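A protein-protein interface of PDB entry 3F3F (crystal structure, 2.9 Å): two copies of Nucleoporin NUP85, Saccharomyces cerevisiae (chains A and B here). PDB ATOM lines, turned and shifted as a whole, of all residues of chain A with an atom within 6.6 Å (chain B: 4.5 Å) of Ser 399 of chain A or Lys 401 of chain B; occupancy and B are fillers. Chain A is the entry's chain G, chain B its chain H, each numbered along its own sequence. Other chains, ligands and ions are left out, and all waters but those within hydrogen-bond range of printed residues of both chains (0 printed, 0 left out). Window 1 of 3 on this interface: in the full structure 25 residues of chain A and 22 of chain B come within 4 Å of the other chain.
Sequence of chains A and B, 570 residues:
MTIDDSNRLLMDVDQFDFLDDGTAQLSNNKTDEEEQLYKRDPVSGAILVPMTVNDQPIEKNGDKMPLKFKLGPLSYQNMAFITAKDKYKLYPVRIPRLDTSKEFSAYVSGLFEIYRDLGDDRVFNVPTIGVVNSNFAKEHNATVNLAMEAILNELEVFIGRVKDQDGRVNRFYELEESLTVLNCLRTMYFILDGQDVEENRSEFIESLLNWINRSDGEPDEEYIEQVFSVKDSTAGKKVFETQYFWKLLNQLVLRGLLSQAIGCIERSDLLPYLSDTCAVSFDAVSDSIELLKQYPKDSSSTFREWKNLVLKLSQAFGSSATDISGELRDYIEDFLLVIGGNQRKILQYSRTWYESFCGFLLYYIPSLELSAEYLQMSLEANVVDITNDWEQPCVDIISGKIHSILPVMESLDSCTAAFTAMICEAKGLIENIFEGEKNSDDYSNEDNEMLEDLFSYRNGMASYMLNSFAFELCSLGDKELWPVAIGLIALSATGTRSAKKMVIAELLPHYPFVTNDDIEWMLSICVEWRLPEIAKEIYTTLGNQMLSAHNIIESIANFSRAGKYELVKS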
ATOM      1  N   MET A 188      -5.341  26.297  -2.142  1.00  0.00           N
ATOM      2  CA  MET A 188      -4.466  25.645  -3.089  1.00  0.00           C
ATOM      3  C   MET A 188      -4.282  26.287  -4.452  1.00  0.00           C
ATOM      4  O   MET A 188      -3.307  25.984  -5.134  1.00  0.00           O
ATOM      5  CB  MET A 188      -4.939  24.218  -3.286  1.00  0.00           C
ATOM      6  CG  MET A 188      -5.074  23.448  -2.007  1.00  0.00           C
ATOM      7  SD  MET A 188      -3.473  23.207  -1.285  1.00  0.00           S
ATOM      8  CE  MET A 188      -2.662  22.125  -2.535  1.00  0.00           C
ATOM      9  N   TYR A 189      -5.195  27.159  -4.869  1.00  0.00           N
ATOM     10  CA  TYR A 189      -5.059  27.769  -6.196  1.00  0.00           C
ATOM     11  C   TYR A 189      -5.321  29.272  -6.302  1.00  0.00           C
ATOM     12  O   TYR A 189      -5.012  29.895  -7.325  1.00  0.00           O
ATOM     13  CB  TYR A 189      -5.967  27.046  -7.198  1.00  0.00           C
ATOM     14  CG  TYR A 189      -5.622  25.597  -7.400  1.00  0.00           C
ATOM     15  CD1 TYR A 189      -6.046  24.632  -6.494  1.00  0.00           C
ATOM     16  CD2 TYR A 189      -4.815  25.196  -8.461  1.00  0.00           C
ATOM     17  CE1 TYR A 189      -5.668  23.308  -6.634  1.00  0.00           C
ATOM     18  CE2 TYR A 189      -4.430  23.873  -8.607  1.00  0.00           C
ATOM     19  CZ  TYR A 189      -4.857  22.939  -7.687  1.00  0.00           C
ATOM     20  OH  TYR A 189      -4.440  21.639  -7.789  1.00  0.00           O
ATOM     21  N   ALA A 372       2.041  16.218  -3.204  1.00  0.00           N
ATOM     22  CA  ALA A 372       1.768  14.929  -3.814  1.00  0.00           C
ATOM     23  C   ALA A 372       2.185  13.808  -2.855  1.00  0.00           C
ATOM     24  O   ALA A 372       1.438  12.857  -2.607  1.00  0.00           O
ATOM     25  CB  ALA A 372       2.537  14.831  -5.113  1.00  0.00           C
ATOM     26  N   LEU A 375       0.252  14.062   0.692  1.00  0.00           N
ATOM     27  CA  LEU A 375      -1.074  13.474   0.581  1.00  0.00           C
ATOM     28  C   LEU A 375      -1.011  11.957   0.592  1.00  0.00           C
ATOM     29  O   LEU A 375      -1.792  11.310   1.279  1.00  0.00           O
ATOM     30  CB  LEU A 375      -1.748  13.956  -0.702  1.00  0.00           C
ATOM     31  CG  LEU A 375      -3.216  13.576  -0.901  1.00  0.00           C
ATOM     32  CD1 LEU A 375      -4.071  14.191   0.183  1.00  0.00           C
ATOM     33  CD2 LEU A 375      -3.672  14.067  -2.241  1.00  0.00           C
ATOM     34  N   GLN A 392     -13.318  13.759   0.338  1.00  0.00           N
ATOM     35  CA  GLN A 392     -12.873  13.345  -0.987  1.00  0.00           C
ATOM     36  C   GLN A 392     -12.627  14.509  -1.946  1.00  0.00           C
ATOM     37  O   GLN A 392     -11.616  14.541  -2.621  1.00  0.00           O
ATOM     38  CB  GLN A 392     -13.861  12.370  -1.611  1.00  0.00           C
ATOM     39  CG  GLN A 392     -13.358  11.795  -2.906  1.00  0.00           C
ATOM     40  CD  GLN A 392     -12.004  11.136  -2.748  1.00  0.00           C
ATOM     41  OE1 GLN A 392     -11.828  10.241  -1.920  1.00  0.00           O
ATOM     42  NE2 GLN A 392     -11.036  11.571  -3.547  1.00  0.00           N
ATOM     43  N   CYS A 394     -11.752  17.440  -1.325  1.00  0.00           N
ATOM     44  CA  CYS A 394     -10.524  18.107  -0.916  1.00  0.00           C
ATOM     45  C   CYS A 394      -9.317  17.298  -1.377  1.00  0.00           C
ATOM     46  O   CYS A 394      -8.324  17.854  -1.861  1.00  0.00           O
ATOM     47  CB  CYS A 394     -10.491  18.297   0.601  1.00  0.00           C
ATOM     48  SG  CYS A 394     -11.460  19.726   1.191  1.00  0.00           S
ATOM     49  N   VAL A 395      -9.403  15.980  -1.229  1.00  0.00           N
ATOM     50  CA  VAL A 395      -8.322  15.117  -1.678  1.00  0.00           C
ATOM     51  C   VAL A 395      -8.128  15.356  -3.174  1.00  0.00           C
ATOM     52  O   VAL A 395      -6.998  15.454  -3.650  1.00  0.00           O
ATOM     53  CB  VAL A 395      -8.646  13.632  -1.434  1.00  0.00           C
ATOM     54  CG1 VAL A 395      -7.729  12.762  -2.249  1.00  0.00           C
ATOM     55  CG2 VAL A 395      -8.482  13.308   0.036  1.00  0.00           C
ATOM     56  N   ASP A 396      -9.230  15.472  -3.912  1.00  0.00           N
ATOM     57  CA  ASP A 396      -9.147  15.706  -5.342  1.00  0.00           C
ATOM     58  C   ASP A 396      -8.504  17.055  -5.638  1.00  0.00           C
ATOM     59  O   ASP A 396      -7.631  17.155  -6.507  1.00  0.00           O
ATOM     60  CB  ASP A 396     -10.530  15.643  -5.989  1.00  0.00           C
ATOM     61  CG  ASP A 396     -11.141  14.251  -5.946  1.00  0.00           C
ATOM     62  OD1 ASP A 396     -10.390  13.252  -6.084  1.00  0.00           O
ATOM     63  OD2 ASP A 396     -12.383  14.158  -5.791  1.00  0.00           O
ATOM     64  N   ILE A 397      -8.927  18.091  -4.918  1.00  0.00           N
ATOM     65  CA  ILE A 397      -8.372  19.428  -5.121  1.00  0.00           C
ATOM     66  C   ILE A 397      -6.865  19.353  -4.976  1.00  0.00           C
ATOM     67  O   ILE A 397      -6.112  19.603  -5.919  1.00  0.00           O
ATOM     68  CB  ILE A 397      -8.922  20.443  -4.084  1.00  0.00           C
ATOM     69  CG1 ILE A 397     -10.417  20.669  -4.317  1.00  0.00           C
ATOM     70  CG2 ILE A 397      -8.143  21.765  -4.171  1.00  0.00           C
ATOM     71  CD1 ILE A 397     -11.062  21.566  -3.313  1.00  0.00           C
ATOM     72  N   ILE A 398      -6.440  18.987  -3.775  1.00  0.00           N
ATOM     73  CA  ILE A 398      -5.027  18.860  -3.466  1.00  0.00           C
ATOM     74  C   ILE A 398      -4.312  18.054  -4.531  1.00  0.00           C
ATOM     75  O   ILE A 398      -3.254  18.455  -5.005  1.00  0.00           O
ATOM     76  CB  ILE A 398      -4.811  18.179  -2.095  1.00  0.00           C
ATOM     77  CG1 ILE A 398      -5.400  19.054  -0.985  1.00  0.00           C
ATOM     78  CG2 ILE A 398      -3.338  17.938  -1.862  1.00  0.00           C
ATOM     79  CD1 ILE A 398      -5.334  18.432   0.395  1.00  0.00           C
ATOM     80  N   SER A 399      -4.892  16.934  -4.937  1.00  0.00           N
ATOM     81  CA  SER A 399      -4.208  16.125  -5.916  1.00  0.00           C
ATOM     82  C   SER A 399      -4.400  16.517  -7.372  1.00  0.00           C
ATOM     83  O   SER A 399      -4.227  15.688  -8.267  1.00  0.00           O
ATOM     84  CB  SER A 399      -4.533  14.646  -5.725  1.00  0.00           C
ATOM     85  OG  SER A 399      -5.846  14.354  -6.119  1.00  0.00           O
ATOM     86  N   GLY A 400      -4.763  17.768  -7.632  1.00  0.00           N
ATOM     87  CA  GLY A 400      -4.872  18.188  -9.015  1.00  0.00           C
ATOM     88  C   GLY A 400      -6.146  18.004  -9.805  1.00  0.00           C
ATOM     89  O   GLY A 400      -6.386  18.792 -10.716  1.00  0.00           O
ATOM     90  N   LYS A 401      -6.962  16.990  -9.524  1.00  0.00           N
ATOM     91  CA  LYS A 401      -8.188  16.873 -10.316  1.00  0.00           C
ATOM     92  C   LYS A 401      -9.360  17.635  -9.716  1.00  0.00           C
ATOM     93  O   LYS A 401     -10.191  17.090  -8.995  1.00  0.00           O
ATOM     94  CB  LYS A 401      -8.564  15.409 -10.607  1.00  0.00           C
ATOM     95  CG  LYS A 401      -8.551  14.417  -9.473  1.00  0.00           C
ATOM     96  CD  LYS A 401      -9.046  13.074 -10.018  1.00  0.00           C
ATOM     97  CE  LYS A 401      -9.274  12.032  -8.934  1.00  0.00           C
ATOM     98  NZ  LYS A 401     -10.272  11.025  -9.413  1.00  0.00           N
ATOM     99  N   ILE A 402      -9.395  18.922 -10.050  1.00  0.00           N
ATOM    100  CA  ILE A 402     -10.407  19.855  -9.591  1.00  0.00           C
ATOM    101  C   ILE A 402     -11.787  19.565 -10.148  1.00  0.00           C
ATOM    102  O   ILE A 402     -12.774  19.531  -9.416  1.00  0.00           O
ATOM    103  CB  ILE A 402     -10.016  21.286  -9.984  1.00  0.00           C
ATOM    104  CG1 ILE A 402      -8.769  21.707  -9.203  1.00  0.00           C
ATOM    105  CG2 ILE A 402     -11.173  22.237  -9.726  1.00  0.00           C
ATOM    106  CD1 ILE A 402      -8.301  23.103  -9.522  1.00  0.00           C
ATOM    107  N   HIS A 403     -11.849  19.358 -11.455  1.00  0.00           N
ATOM    108  CA  HIS A 403     -13.109  19.090 -12.126  1.00  0.00           C
ATOM    109  C   HIS A 403     -14.032  18.123 -11.396  1.00  0.00           C
ATOM    110  O   HIS A 403     -15.247  18.283 -11.438  1.00  0.00           O
ATOM    111  CB  HIS A 403     -12.846  18.587 -13.553  1.00  0.00           C
ATOM    112  CG  HIS A 403     -12.311  17.188 -13.627  1.00  0.00           C
ATOM    113  ND1 HIS A 403     -11.352  16.709 -12.763  1.00  0.00           N
ATOM    114  CD2 HIS A 403     -12.589  16.172 -14.478  1.00  0.00           C
ATOM    115  CE1 HIS A 403     -11.065  15.457 -13.074  1.00  0.00           C
ATOM    116  NE2 HIS A 403     -11.801  15.107 -14.112  1.00  0.00           N
ATOM    117  N   ASP B 396      -5.930   7.121 -13.673  1.00  0.00           N
ATOM    118  CA  ASP B 396      -5.366   8.417 -13.294  1.00  0.00           C
ATOM    119  C   ASP B 396      -5.082   9.278 -14.534  1.00  0.00           C
ATOM    120  O   ASP B 396      -5.407  10.469 -14.570  1.00  0.00           O
ATOM    121  CB  ASP B 396      -4.069   8.245 -12.476  1.00  0.00           C
ATOM    122  CG  ASP B 396      -4.302   7.611 -11.096  1.00  0.00           C
ATOM    123  OD1 ASP B 396      -5.338   7.913 -10.449  1.00  0.00           O
ATOM    124  OD2 ASP B 396      -3.430   6.826 -10.651  1.00  0.00           O
ATOM    125  N   ILE B 397      -4.464   8.673 -15.544  1.00  0.00           N
ATOM    126  CA  ILE B 397      -4.147   9.394 -16.778  1.00  0.00           C
ATOM    127  C   ILE B 397      -5.437  10.012 -17.315  1.00  0.00           C
ATOM    128  O   ILE B 397      -5.571  11.237 -17.407  1.00  0.00           O
ATOM    129  CB  ILE B 397      -3.566   8.439 -17.871  1.00  0.00           C
ATOM    130  CG1 ILE B 397      -2.192   7.920 -17.439  1.00  0.00           C
ATOM    131  CG2 ILE B 397      -3.488   9.162 -19.224  1.00  0.00           C
ATOM    132  CD1 ILE B 397      -1.595   6.902 -18.391  1.00  0.00           C
ATOM    133  N   SER B 399      -8.221  10.493 -16.016  1.00  0.00           N
ATOM    134  CA  SER B 399      -8.817  11.497 -15.144  1.00  0.00           C
ATOM    135  C   SER B 399      -7.956  12.713 -14.799  1.00  0.00           C
ATOM    136  O   SER B 399      -8.197  13.382 -13.800  1.00  0.00           O
ATOM    137  CB  SER B 399      -9.368  10.852 -13.857  1.00  0.00           C
ATOM    138  OG  SER B 399      -8.345  10.447 -12.978  1.00  0.00           O
ATOM    139  N   GLY B 400      -6.960  13.008 -15.620  1.00  0.00           N
ATOM    140  CA  GLY B 400      -6.163  14.191 -15.363  1.00  0.00           C
ATOM    141  C   GLY B 400      -4.969  14.159 -14.427  1.00  0.00           C
ATOM    142  O   GLY B 400      -4.058  14.966 -14.617  1.00  0.00           O
ATOM    143  N   LYS B 401      -4.935  13.292 -13.415  1.00  0.00           N
ATOM    144  CA  LYS B 401      -3.756  13.298 -12.552  1.00  0.00           C
ATOM    145  C   LYS B 401      -2.668  12.343 -13.024  1.00  0.00           C
ATOM    146  O   LYS B 401      -2.552  11.203 -12.587  1.00  0.00           O
ATOM    147  CB  LYS B 401      -4.112  13.065 -11.071  1.00  0.00           C
ATOM    148  CG  LYS B 401      -5.008  11.902 -10.719  1.00  0.00           C
ATOM    149  CD  LYS B 401      -5.096  11.832  -9.190  1.00  0.00           C
ATOM    150  CE  LYS B 401      -5.848  10.600  -8.684  1.00  0.00           C
ATOM    151  NZ  LYS B 401      -5.438  10.300  -7.272  1.00  0.00           N
ATOM    152  N   ILE B 402      -1.871  12.864 -13.944  1.00  0.00           N
ATOM    153  CA  ILE B 402      -0.769  12.154 -14.563  1.00  0.00           C
ATOM    154  C   ILE B 402       0.360  11.878 -13.592  1.00  0.00           C
ATOM    155  O   ILE B 402       0.849  10.754 -13.509  1.00  0.00           O
ATOM    156  CB  ILE B 402      -0.203  12.972 -15.747  1.00  0.00           C
ATOM    157  CG1 ILE B 402      -1.237  13.035 -16.867  1.00  0.00           C
ATOM    158  CG2 ILE B 402       1.091  12.365 -16.242  1.00  0.00           C
ATOM    159  CD1 ILE B 402      -0.794  13.832 -18.074  1.00  0.00           C
ATOM    160  N   HIS B 403       0.773  12.909 -12.866  1.00  0.00           N
ATOM    161  CA  HIS B 403       1.872  12.784 -11.920  1.00  0.00           C
ATOM    162  C   HIS B 403       1.850  11.500 -11.082  1.00  0.00           C
ATOM    163  O   HIS B 403       2.899  10.947 -10.777  1.00  0.00           O
ATOM    164  CB  HIS B 403       1.917  14.015 -11.010  1.00  0.00           C
ATOM    165  CG  HIS B 403       0.820  14.065  -9.995  1.00  0.00           C
ATOM    166  ND1 HIS B 403      -0.483  13.733 -10.294  1.00  0.00           N
ATOM    167  CD2 HIS B 403       0.829  14.422  -8.687  1.00  0.00           C
ATOM    168  CE1 HIS B 403      -1.231  13.880  -9.214  1.00  0.00           C
ATOM    169  NE2 HIS B 403      -0.459  14.297  -8.224  1.00  0.00           N
ATOM    170  N   SER B 404       0.670  10.996 -10.737  1.00  0.00           N
ATOM    171  CA  SER B 404       0.609   9.795  -9.914  1.00  0.00           C
ATOM    172  C   SER B 404       0.724   8.443 -10.626  1.00  0.00           C
ATOM    173  O   SER B 404       0.286   7.416 -10.098  1.00  0.00           O
ATOM    174  CB  SER B 404      -0.640   9.823  -9.008  1.00  0.00           C
ATOM    175  OG  SER B 404      -1.832  10.105  -9.720  1.00  0.00           O
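O of Val 395 of chain A lies within hydrogen-bond range of OG of Ser 399 of chain A.
OG of Ser 399 of chain A sits at hydrogen-bond distance from O of Asp 396 of chain A (3.3 Å).
The backbone carbonyl oxygen of Asp 396 of chain A sits at hydrogen-bond distance from the backbone NH of Lys 401 of chain A (3.1 Å).
The backbone carbonyl oxygen of Asp 396 of chain B is in hydrogen-bond range of the side-chain hydroxyl of Ser 399 of chain B, at 3.3 Å.
OD1 of Asp 396 of chain B lies within salt-bridge range of NZ of Lys 401 of chain B (3.98 Å).
The side-chain hydroxyl of Ser 404 of chain B sits at hydrogen-bond distance from the backbone carbonyl oxygen of Lys 401 of chain B (3.2 Å).
Among the printed residues, merely in contact across the chains: His 403 of chain A with Ser 399 of chain B (3.6 Å), Ser 399 of chain A with His 403 of chain B (3.6 Å), Lys 401 of chain A with Lys 401 of chain B (3.7 Å), Lys 401 of chain A with Ser 399 of chain B (3.8 Å), Ser 399 of chain A with Lys 401 of chain B (3.8 Å) and Ala 372 of chain A with His 403 of chain B (3.98 Å).
Ser 399 of chain A touches two residues of chain B.
Lys 401 of chain B touches just these residues of chain A: Ser 399 (3.8 Å) and Lys 401 (3.7 Å).
Printed residues of chain A within 4 Å of Ser 399 of chain B: Lys 401 and His 403.
Printed residues of chain A within 4 Å of His 403 of chain B: Ala 372 (3.98 Å) and Ser 399 (3.6 Å).
Of the printed residues of chain B, Ala 372 of chain A touches His 403.
Of the printed residues of chain B, Lys 401 of chain A touches Ser 399 and Lys 401.
Of the printed residues of chain B, His 403 of chain A touches Ser 399 (3.6 Å).
The nearest printed residue of chain B that does not touch Ser 399 of chain A is Ser 404 of chain B (6.2 Å).
The nearest residue of chain A that does not touch Lys 401 of chain B is Gly 400 of chain A (5.5 Å).
Hydrophobic or aromatic side chains of chain A that line the printed part of chain B: Ala 372 and His 403.
Of the 8 printed residues of chain B, 3 touch a printed residue of chain A.
Hydrophobic or aromatic side chains of chain B that line the printed part of chain A: His 403.
Among the printed residues, no Asp or Glu carboxylate lies within 4 Å of a Lys or Arg side-chain nitrogen of the other chain.
Ser 399 of chain A touches Lys 401 of chain B, and with the chains exchanged Lys 401 of chain A touches Ser 399 of chain B.
Ser 399 of chain A touches His 403 of chain B, and with the chains exchanged His 403 of chain A touches Ser 399 of chain B.
Lys 401 of chain A touches its own counterpart, Lys 401 of chain B.
Positions printed for both chains: 396, 397, 399, 400, 401, 402 and 403.
Of the 6 pairs that touch across the chains among the printed residues, 5 have their exchanged pair printed and touching as well.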
